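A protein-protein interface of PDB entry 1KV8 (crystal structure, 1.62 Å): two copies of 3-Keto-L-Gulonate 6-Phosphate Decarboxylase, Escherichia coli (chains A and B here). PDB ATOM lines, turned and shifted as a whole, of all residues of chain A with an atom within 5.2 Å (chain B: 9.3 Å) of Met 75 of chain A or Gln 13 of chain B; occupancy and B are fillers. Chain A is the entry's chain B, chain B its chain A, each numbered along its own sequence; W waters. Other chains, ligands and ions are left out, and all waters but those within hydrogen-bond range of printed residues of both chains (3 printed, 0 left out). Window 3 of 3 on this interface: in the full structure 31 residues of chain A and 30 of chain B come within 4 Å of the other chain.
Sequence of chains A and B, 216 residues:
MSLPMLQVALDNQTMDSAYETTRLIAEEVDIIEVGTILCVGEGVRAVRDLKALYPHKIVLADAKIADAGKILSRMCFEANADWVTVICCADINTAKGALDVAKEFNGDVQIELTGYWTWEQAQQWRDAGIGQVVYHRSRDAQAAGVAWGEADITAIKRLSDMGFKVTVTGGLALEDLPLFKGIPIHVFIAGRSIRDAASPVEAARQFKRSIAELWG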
ATOM      1  N   VAL A  44      29.229   9.340   3.276  1.00  0.00           N
ATOM      2  CA  VAL A  44      30.061   8.570   4.191  1.00  0.00           C
ATOM      3  C   VAL A  44      29.826   7.057   4.197  1.00  0.00           C
ATOM      4  O   VAL A  44      30.634   6.304   4.745  1.00  0.00           O
ATOM      5  CB  VAL A  44      29.939   9.140   5.623  1.00  0.00           C
ATOM      6  CG1 VAL A  44      28.583   8.805   6.208  1.00  0.00           C
ATOM      7  CG2 VAL A  44      31.075   8.630   6.485  1.00  0.00           C
ATOM      8  N   LYS A  70      35.469  19.007  13.662  1.00  0.00           N
ATOM      9  CA  LYS A  70      34.958  18.021  14.605  1.00  0.00           C
ATOM     10  C   LYS A  70      33.778  17.240  14.028  1.00  0.00           C
ATOM     11  O   LYS A  70      33.746  16.010  14.087  1.00  0.00           O
ATOM     12  CB  LYS A  70      34.525  18.707  15.907  1.00  0.00           C
ATOM     13  CG  LYS A  70      33.935  17.755  16.938  1.00  0.00           C
ATOM     14  CD  LYS A  70      33.533  18.484  18.219  1.00  0.00           C
ATOM     15  CE  LYS A  70      32.440  19.517  17.960  1.00  0.00           C
ATOM     16  NZ  LYS A  70      32.007  20.196  19.218  1.00  0.00           N
ATOM     17  N   ILE A  71      32.808  17.957  13.471  1.00  0.00           N
ATOM     18  CA  ILE A  71      31.626  17.313  12.914  1.00  0.00           C
ATOM     19  C   ILE A  71      31.951  16.382  11.751  1.00  0.00           C
ATOM     20  O   ILE A  71      31.567  15.212  11.762  1.00  0.00           O
ATOM     21  CB  ILE A  71      30.591  18.361  12.444  1.00  0.00           C
ATOM     22  CG1 ILE A  71      30.068  19.146  13.653  1.00  0.00           C
ATOM     23  CG2 ILE A  71      29.435  17.666  11.724  1.00  0.00           C
ATOM     24  CD1 ILE A  71      29.214  20.352  13.284  1.00  0.00           C
ATOM     25  N   LEU A  72      32.664  16.897  10.756  1.00  0.00           N
ATOM     26  CA  LEU A  72      33.004  16.088   9.596  1.00  0.00           C
ATOM     27  C   LEU A  72      33.919  14.910   9.915  1.00  0.00           C
ATOM     28  O   LEU A  72      33.731  13.819   9.385  1.00  0.00           O
ATOM     29  CB  LEU A  72      33.613  16.965   8.497  1.00  0.00           C
ATOM     30  CG  LEU A  72      32.574  17.827   7.765  1.00  0.00           C
ATOM     31  CD1 LEU A  72      33.265  18.826   6.861  1.00  0.00           C
ATOM     32  CD2 LEU A  72      31.641  16.926   6.958  1.00  0.00           C
ATOM     33  N   SER A  73      34.914  15.126  10.771  1.00  0.00           N
ATOM     34  CA  SER A  73      35.821  14.042  11.118  1.00  0.00           C
ATOM     35  C   SER A  73      35.078  12.957  11.889  1.00  0.00           C
ATOM     36  O   SER A  73      35.322  11.770  11.685  1.00  0.00           O
ATOM     37  CB  SER A  73      37.007  14.560  11.944  1.00  0.00           C
ATOM     38  OG  SER A  73      36.596  15.045  13.208  1.00  0.00           O
ATOM     39  N   ARG A  74      34.159  13.357  12.765  1.00  0.00           N
ATOM     40  CA  ARG A  74      33.403  12.376  13.536  1.00  0.00           C
ATOM     41  C   ARG A  74      32.535  11.530  12.608  1.00  0.00           C
ATOM     42  O   ARG A  74      32.403  10.323  12.803  1.00  0.00           O
ATOM     43  CB  ARG A  74      32.531  13.066  14.592  1.00  0.00           C
ATOM     44  CG  ARG A  74      31.871  12.098  15.565  1.00  0.00           C
ATOM     45  CD  ARG A  74      31.139  12.833  16.682  1.00  0.00           C
ATOM     46  NE  ARG A  74      32.046  13.622  17.514  1.00  0.00           N
ATOM     47  CZ  ARG A  74      32.940  13.107  18.352  1.00  0.00           C
ATOM     48  NH1 ARG A  74      33.057  11.793  18.484  1.00  0.00           N
ATOM     49  NH2 ARG A  74      33.723  13.909  19.060  1.00  0.00           N
ATOM     50  N   MET A  75      31.947  12.160  11.595  1.00  0.00           N
ATOM     51  CA  MET A  75      31.116  11.425  10.648  1.00  0.00           C
ATOM     52  C   MET A  75      31.943  10.337   9.962  1.00  0.00           C
ATOM     53  O   MET A  75      31.487   9.200   9.801  1.00  0.00           O
ATOM     54  CB  MET A  75      30.536  12.383   9.606  1.00  0.00           C
ATOM     55  CG  MET A  75      29.481  13.314  10.174  1.00  0.00           C
ATOM     56  SD  MET A  75      28.979  14.603   9.020  1.00  0.00           S
ATOM     57  CE  MET A  75      28.169  13.619   7.757  1.00  0.00           C
ATOM     58  N   CYS A  76      33.168  10.682   9.580  1.00  0.00           N
ATOM     59  CA  CYS A  76      34.050   9.729   8.908  1.00  0.00           C
ATOM     60  C   CYS A  76      34.537   8.628   9.841  1.00  0.00           C
ATOM     61  O   CYS A  76      34.557   7.450   9.471  1.00  0.00           O
ATOM     62  CB  CYS A  76      35.257  10.455   8.304  1.00  0.00           C
ATOM     63  SG  CYS A  76      34.855  11.554   6.922  1.00  0.00           S
ATOM     64  N   PHE A  77      34.929   9.005  11.054  1.00  0.00           N
ATOM     65  CA  PHE A  77      35.423   8.019  12.001  1.00  0.00           C
ATOM     66  C   PHE A  77      34.330   7.105  12.541  1.00  0.00           C
ATOM     67  O   PHE A  77      34.594   5.945  12.850  1.00  0.00           O
ATOM     68  CB  PHE A  77      36.195   8.713  13.126  1.00  0.00           C
ATOM     69  CG  PHE A  77      37.556   9.189  12.699  1.00  0.00           C
ATOM     70  CD1 PHE A  77      38.517   8.274  12.276  1.00  0.00           C
ATOM     71  CD2 PHE A  77      37.866  10.543  12.674  1.00  0.00           C
ATOM     72  CE1 PHE A  77      39.768   8.702  11.833  1.00  0.00           C
ATOM     73  CE2 PHE A  77      39.114  10.980  12.230  1.00  0.00           C
ATOM     74  CZ  PHE A  77      40.065  10.056  11.809  1.00  0.00           C
ATOM     75  N   GLU A  78      33.102   7.611  12.643  1.00  0.00           N
ATOM     76  CA  GLU A  78      31.999   6.775  13.101  1.00  0.00           C
ATOM     77  C   GLU A  78      31.698   5.758  12.001  1.00  0.00           C
ATOM     78  O   GLU A  78      31.120   4.700  12.263  1.00  0.00           O
ATOM     79  CB  GLU A  78      30.758   7.616  13.406  1.00  0.00           C
ATOM     80  CG  GLU A  78      30.913   8.501  14.640  1.00  0.00           C
ATOM     81  CD  GLU A  78      29.635   9.229  15.008  1.00  0.00           C
ATOM     82  OE1 GLU A  78      28.864   9.581  14.094  1.00  0.00           O
ATOM     83  OE2 GLU A  78      29.408   9.462  16.214  1.00  0.00           O
ATOM     84  N   ALA A  79      32.097   6.094  10.772  1.00  0.00           N
ATOM     85  CA  ALA A  79      31.923   5.210   9.620  1.00  0.00           C
ATOM     86  C   ALA A  79      33.129   4.267   9.506  1.00  0.00           C
ATOM     87  O   ALA A  79      33.291   3.555   8.508  1.00  0.00           O
ATOM     88  CB  ALA A  79      31.760   6.031   8.338  1.00  0.00           C
ATOM     89  N   LEU B  10      21.738  23.942   5.032  1.00  0.00           N
ATOM     90  CA  LEU B  10      21.312  22.670   5.591  1.00  0.00           C
ATOM     91  C   LEU B  10      22.560  21.857   5.907  1.00  0.00           C
ATOM     92  O   LEU B  10      23.066  21.111   5.064  1.00  0.00           O
ATOM     93  CB  LEU B  10      20.418  21.916   4.604  1.00  0.00           C
ATOM     94  CG  LEU B  10      19.127  22.638   4.208  1.00  0.00           C
ATOM     95  CD1 LEU B  10      18.404  21.828   3.147  1.00  0.00           C
ATOM     96  CD2 LEU B  10      18.232  22.839   5.435  1.00  0.00           C
ATOM     97  N   ASP B  11      23.071  22.034   7.121  1.00  0.00           N
ATOM     98  CA  ASP B  11      24.247  21.307   7.571  1.00  0.00           C
ATOM     99  C   ASP B  11      23.815  20.110   8.396  1.00  0.00           C
ATOM    100  O   ASP B  11      24.247  19.923   9.531  1.00  0.00           O
ATOM    101  CB  ASP B  11      25.162  22.222   8.388  1.00  0.00           C
ATOM    102  CG  ASP B  11      25.974  23.145   7.511  1.00  0.00           C
ATOM    103  OD1 ASP B  11      26.531  22.649   6.509  1.00  0.00           O
ATOM    104  OD2 ASP B  11      26.065  24.351   7.821  1.00  0.00           O
ATOM    105  N   ASN B  12      22.947  19.302   7.802  1.00  0.00           N
ATOM    106  CA  ASN B  12      22.414  18.108   8.442  1.00  0.00           C
ATOM    107  C   ASN B  12      23.171  16.896   7.923  1.00  0.00           C
ATOM    108  O   ASN B  12      23.713  16.931   6.821  1.00  0.00           O
ATOM    109  CB  ASN B  12      20.927  17.988   8.108  1.00  0.00           C
ATOM    110  CG  ASN B  12      20.147  19.225   8.505  1.00  0.00           C
ATOM    111  OD1 ASN B  12      19.553  19.282   9.584  1.00  0.00           O
ATOM    112  ND2 ASN B  12      20.160  20.233   7.641  1.00  0.00           N
ATOM    113  N   GLN B  13      23.204  15.821   8.705  1.00  0.00           N
ATOM    114  CA  GLN B  13      23.920  14.620   8.293  1.00  0.00           C
ATOM    115  C   GLN B  13      23.081  13.656   7.466  1.00  0.00           C
ATOM    116  O   GLN B  13      23.626  12.786   6.790  1.00  0.00           O
ATOM    117  CB  GLN B  13      24.487  13.902   9.518  1.00  0.00           C
ATOM    118  CG  GLN B  13      25.345  14.808  10.381  1.00  0.00           C
ATOM    119  CD  GLN B  13      26.121  14.061  11.446  1.00  0.00           C
ATOM    120  OE1 GLN B  13      26.667  14.670  12.364  1.00  0.00           O
ATOM    121  NE2 GLN B  13      26.185  12.740  11.325  1.00  0.00           N
ATOM    122  N   THR B  14      21.758  13.809   7.519  1.00  0.00           N
ATOM    123  CA  THR B  14      20.849  12.954   6.757  1.00  0.00           C
ATOM    124  C   THR B  14      19.717  13.777   6.151  1.00  0.00           C
ATOM    125  O   THR B  14      19.406  14.871   6.637  1.00  0.00           O
ATOM    126  CB  THR B  14      20.221  11.852   7.638  1.00  0.00           C
ATOM    127  OG1 THR B  14      19.494  12.455   8.714  1.00  0.00           O
ATOM    128  CG2 THR B  14      21.300  10.940   8.205  1.00  0.00           C
ATOM    129  N   MET B  15      19.110  13.253   5.088  1.00  0.00           N
ATOM    130  CA  MET B  15      18.016  13.948   4.417  1.00  0.00           C
ATOM    131  C   MET B  15      16.827  14.165   5.337  1.00  0.00           C
ATOM    132  O   MET B  15      16.240  15.250   5.345  1.00  0.00           O
ATOM    133  CB  MET B  15      17.532  13.175   3.183  1.00  0.00           C
ATOM    134  CG  MET B  15      18.556  12.999   2.075  1.00  0.00           C
ATOM    135  SD  MET B  15      19.431  14.509   1.659  1.00  0.00           S
ATOM    136  CE  MET B  15      18.109  15.560   1.011  1.00  0.00           C
ATOM    137  N   ASP B  16      16.455  13.143   6.106  1.00  0.00           N
ATOM    138  CA  ASP B  16      15.305  13.304   6.988  1.00  0.00           C
ATOM    139  C   ASP B  16      15.516  14.418   8.010  1.00  0.00           C
ATOM    140  O   ASP B  16      14.564  15.115   8.369  1.00  0.00           O
ATOM    141  CB  ASP B  16      14.916  11.973   7.665  1.00  0.00           C
ATOM    142  CG  ASP B  16      15.979  11.439   8.605  1.00  0.00           C
ATOM    143  OD1 ASP B  16      17.128  11.232   8.171  1.00  0.00           O
ATOM    144  OD2 ASP B  16      15.650  11.205   9.787  1.00  0.00           O
ATOM    145  N   SER B  17      16.758  14.602   8.462  1.00  0.00           N
ATOM    146  CA  SER B  17      17.074  15.675   9.408  1.00  0.00           C
ATOM    147  C   SER B  17      16.912  17.019   8.690  1.00  0.00           C
ATOM    148  O   SER B  17      16.361  17.970   9.242  1.00  0.00           O
ATOM    149  CB  SER B  17      18.514  15.533   9.921  1.00  0.00           C
ATOM    150  OG  SER B  17      18.888  16.649  10.719  1.00  0.00           O
ATOM    151  N   ALA B  18      17.388  17.094   7.450  1.00  0.00           N
ATOM    152  CA  ALA B  18      17.271  18.323   6.672  1.00  0.00           C
ATOM    153  C   ALA B  18      15.806  18.678   6.427  1.00  0.00           C
ATOM    154  O   ALA B  18      15.429  19.851   6.475  1.00  0.00           O
ATOM    155  CB  ALA B  18      18.004  18.169   5.332  1.00  0.00           C
ATOM    156  N   TYR B  19      14.974  17.670   6.177  1.00  0.00           N
ATOM    157  CA  TYR B  19      13.560  17.921   5.909  1.00  0.00           C
ATOM    158  C   TYR B  19      12.825  18.491   7.116  1.00  0.00           C
ATOM    159  O   TYR B  19      11.810  19.169   6.962  1.00  0.00           O
ATOM    160  CB  TYR B  19      12.870  16.643   5.416  1.00  0.00           C
ATOM    161  CG  TYR B  19      13.451  16.110   4.120  1.00  0.00           C
ATOM    162  CD1 TYR B  19      14.015  16.971   3.179  1.00  0.00           C
ATOM    163  CD2 TYR B  19      13.431  14.743   3.833  1.00  0.00           C
ATOM    164  CE1 TYR B  19      14.550  16.484   1.983  1.00  0.00           C
ATOM    165  CE2 TYR B  19      13.959  14.244   2.639  1.00  0.00           C
ATOM    166  CZ  TYR B  19      14.518  15.122   1.724  1.00  0.00           C
ATOM    167  OH  TYR B  19      15.051  14.639   0.556  1.00  0.00           O
ATOM    168  N   GLY B  35      24.421  21.892   2.588  1.00  0.00           N
ATOM    169  CA  GLY B  35      25.673  22.138   3.275  1.00  0.00           C
ATOM    170  C   GLY B  35      26.705  21.069   3.020  1.00  0.00           C
ATOM    171  O   GLY B  35      26.366  19.945   2.656  1.00  0.00           O
ATOM    172  N   THR B  36      27.973  21.416   3.208  1.00  0.00           N
ATOM    173  CA  THR B  36      29.043  20.453   3.002  1.00  0.00           C
ATOM    174  C   THR B  36      28.791  19.215   3.862  1.00  0.00           C
ATOM    175  O   THR B  36      29.030  18.089   3.433  1.00  0.00           O
ATOM    176  CB  THR B  36      30.403  21.069   3.361  1.00  0.00           C
ATOM    177  OG1 THR B  36      30.559  22.311   2.656  1.00  0.00           O
ATOM    178  CG2 THR B  36      31.535  20.126   2.965  1.00  0.00           C
ATOM    179  N   ILE B  37      28.288  19.431   5.072  1.00  0.00           N
ATOM    180  CA  ILE B  37      27.991  18.327   5.974  1.00  0.00           C
ATOM    181  C   ILE B  37      26.947  17.374   5.379  1.00  0.00           C
ATOM    182  O   ILE B  37      27.070  16.158   5.502  1.00  0.00           O
ATOM    183  CB  ILE B  37      27.532  18.870   7.348  1.00  0.00           C
ATOM    184  CG1 ILE B  37      28.723  19.562   8.028  1.00  0.00           C
ATOM    185  CG2 ILE B  37      26.978  17.742   8.213  1.00  0.00           C
ATOM    186  CD1 ILE B  37      28.370  20.367   9.271  1.00  0.00           C
ATOM    187  N   LEU B  38      25.931  17.917   4.714  1.00  0.00           N
ATOM    188  CA  LEU B  38      24.903  17.071   4.111  1.00  0.00           C
ATOM    189  C   LEU B  38      25.464  16.376   2.869  1.00  0.00           C
ATOM    190  O   LEU B  38      25.110  15.232   2.575  1.00  0.00           O
ATOM    191  CB  LEU B  38      23.668  17.909   3.747  1.00  0.00           C
ATOM    192  CG  LEU B  38      22.444  17.129   3.255  1.00  0.00           C
ATOM    193  CD1 LEU B  38      22.058  16.030   4.251  1.00  0.00           C
ATOM    194  CD2 LEU B  38      21.289  18.098   3.068  1.00  0.00           C
ATOM    195  N   CYS B  39      26.340  17.072   2.150  1.00  0.00           N
ATOM    196  CA  CYS B  39      26.976  16.511   0.958  1.00  0.00           C
ATOM    197  C   CYS B  39      27.789  15.279   1.352  1.00  0.00           C
ATOM    198  O   CYS B  39      27.746  14.246   0.680  1.00  0.00           O
ATOM    199  CB  CYS B  39      27.911  17.534   0.312  1.00  0.00           C
ATOM    200  SG  CYS B  39      27.096  18.853  -0.632  1.00  0.00           S
ATOM    201  N   VAL B  40      28.534  15.395   2.444  1.00  0.00           N
ATOM    202  CA  VAL B  40      29.356  14.286   2.917  1.00  0.00           C
ATOM    203  C   VAL B  40      28.511  13.193   3.555  1.00  0.00           C
ATOM    204  O   VAL B  40      28.840  12.007   3.469  1.00  0.00           O
ATOM    205  CB  VAL B  40      30.416  14.780   3.929  1.00  0.00           C
ATOM    206  CG1 VAL B  40      31.135  13.596   4.571  1.00  0.00           C
ATOM    207  CG2 VAL B  40      31.427  15.652   3.214  1.00  0.00           C
ATOM    208  N   GLY B  41      27.413  13.586   4.186  1.00  0.00           N
ATOM    209  CA  GLY B  41      26.563  12.601   4.821  1.00  0.00           C
ATOM    210  C   GLY B  41      25.747  11.748   3.865  1.00  0.00           C
ATOM    211  O   GLY B  41      25.691  10.524   4.006  1.00  0.00           O
ATOM    212  N   GLU B  42      25.129  12.386   2.877  1.00  0.00           N
ATOM    213  CA  GLU B  42      24.266  11.679   1.935  1.00  0.00           C
ATOM    214  C   GLU B  42      24.758  11.598   0.500  1.00  0.00           C
ATOM    215  O   GLU B  42      24.252  10.793  -0.285  1.00  0.00           O
ATOM    216  CB  GLU B  42      22.880  12.332   1.938  1.00  0.00           C
ATOM    217  CG  GLU B  42      22.156  12.233   3.263  1.00  0.00           C
ATOM    218  CD  GLU B  42      21.391  10.936   3.411  1.00  0.00           C
ATOM    219  OE1 GLU B  42      21.802   9.924   2.802  1.00  0.00           O
ATOM    220  OE2 GLU B  42      20.381  10.925   4.144  1.00  0.00           O
ATOM    221  N   GLY B  43      25.732  12.421   0.143  1.00  0.00           N
ATOM    222  CA  GLY B  43      26.202  12.396  -1.229  1.00  0.00           C
ATOM    223  C   GLY B  43      25.352  13.317  -2.084  1.00  0.00           C
ATOM    224  O   GLY B  43      24.437  13.974  -1.591  1.00  0.00           O
ATOM    225  N   ARG B  45      22.942  12.866  -3.921  1.00  0.00           N
ATOM    226  CA  ARG B  45      21.510  12.614  -3.997  1.00  0.00           C
ATOM    227  C   ARG B  45      20.770  13.711  -3.230  1.00  0.00           C
ATOM    228  O   ARG B  45      19.598  13.976  -3.487  1.00  0.00           O
ATOM    229  CB  ARG B  45      21.160  11.245  -3.406  1.00  0.00           C
ATOM    230  CG  ARG B  45      21.326  11.143  -1.899  1.00  0.00           C
ATOM    231  CD  ARG B  45      20.540   9.960  -1.361  1.00  0.00           C
ATOM    232  NE  ARG B  45      19.119  10.091  -1.671  1.00  0.00           N
ATOM    233  CZ  ARG B  45      18.349   9.088  -2.079  1.00  0.00           C
ATOM    234  NH1 ARG B  45      18.860   7.871  -2.228  1.00  0.00           N
ATOM    235  NH2 ARG B  45      17.072   9.304  -2.347  1.00  0.00           N
ATOM    236  N   ALA B  46      21.459  14.352  -2.289  1.00  0.00           N
ATOM    237  CA  ALA B  46      20.846  15.418  -1.503  1.00  0.00           C
ATOM    238  C   ALA B  46      20.430  16.570  -2.409  1.00  0.00           C
ATOM    239  O   ALA B  46      19.369  17.163  -2.230  1.00  0.00           O
ATOM    240  CB  ALA B  46      21.818  15.921  -0.436  1.00  0.00           C
ATOM    241  N   ARG B 195      17.764  27.002  11.613  1.00  0.00           N
ATOM    242  CA  ARG B 195      17.466  25.606  11.914  1.00  0.00           C
ATOM    243  C   ARG B 195      17.245  25.325  13.398  1.00  0.00           C
ATOM    244  O   ARG B 195      16.323  24.600  13.769  1.00  0.00           O
ATOM    245  CB  ARG B 195      18.592  24.686  11.437  1.00  0.00           C
ATOM    246  CG  ARG B 195      18.931  24.741   9.949  1.00  0.00           C
ATOM    247  CD  ARG B 195      19.706  23.480   9.558  1.00  0.00           C
ATOM    248  NE  ARG B 195      20.758  23.172  10.529  1.00  0.00           N
ATOM    249  CZ  ARG B 195      21.973  23.712  10.527  1.00  0.00           C
ATOM    250  NH1 ARG B 195      22.317  24.588   9.595  1.00  0.00           N
ATOM    251  NH2 ARG B 195      22.838  23.401  11.483  1.00  0.00           N
HETATM  252  O   HOH W   1      28.520  11.926  13.173  1.00  0.00           O
HETATM  253  O   HOH W   2      26.150   8.085   2.826  1.00  0.00           O
HETATM  254  O   HOH W   3      29.336  14.463  13.486  1.00  0.00           O
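The backbone carbonyl oxygen (O) of Val 40 of chain B lies within hydrogen-bond range of the backbone NH (N) of Val 44 of chain A (2.7 Å).
The side-chain sulfur (SG) of Cys 76 of chain A is in hydrogen-bond range of the backbone carbonyl oxygen (O) of Leu 72 of chain A (3.5 Å).
N of Val 44 of chain A touches O of Gly 41 of chain B, at 3.8 Å.
Ile 71 of chain A touches Ile 37 of chain B (CG2 to CD1, 3.8 Å).
Val 40 of chain B touches Leu 72 of chain A (CB to CD2, 3.9 Å).
NE2 of Gln 13 of chain B touches CG of Met 75 of chain A (3.5 Å).
Met 75 of chain A touches Ile 37 of chain B.
Met 75 of chain A touches Gly 41 of chain B (CE to CA, 3.5 Å).
No residue of chain B comes within 4 Å of Cys 76 of chain A.
Asp 11 of chain B touches none of the printed residues of chain A.
Of chain A, only Met 75 comes within 4 Å of Gln 13 of chain B.
Cys 39 of chain B touches none of the printed residues of chain A.
Of the printed residues of chain A, Val 40 of chain B touches Val 44 and Leu 72.
Of the printed residues of chain A, Gly 41 of chain B touches Val 44 (3.8 Å) and Met 75 (3.5 Å).
The nearest residue of chain A that does not touch Gln 13 of chain B is Ile 71 of chain A (4.1 Å).
Of the 11 printed residues of chain A, 4 touch a printed residue of chain B.
Hydrophobic or aromatic side chains of chain A that line the printed part of chain B: Val 44, Ile 71, Leu 72 and Met 75.
Along chain A the printed residues that touch a printed residue of chain B span positions 44 to 75.
Hydrophobic or aromatic side chains of chain B that line the printed part of chain A: Ile 37 and Val 40.
Among the printed residues, no Asp or Glu carboxylate lies within 4 Å of a Lys or Arg side-chain nitrogen of the other chain.
No position is printed for both chains.
Of the 7 pairs that touch across the chains among the printed residues, none has its exchanged pair printed and touching as well.
Water W1 bridges OE1 of Glu 78 of chain A and NE2 of Gln 13 of chain B.
Water W2 bridges O of Gly 41 of chain B (2.7 Å) and N of Val 44 of chain A (3.4 Å).
Water W3 bridges the side-chain amide oxygen (OE1) of Gln 13 of chain B (2.9 Å) and the backbone carbonyl oxygen (O) of Ile 71 of chain A (2.9 Å).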
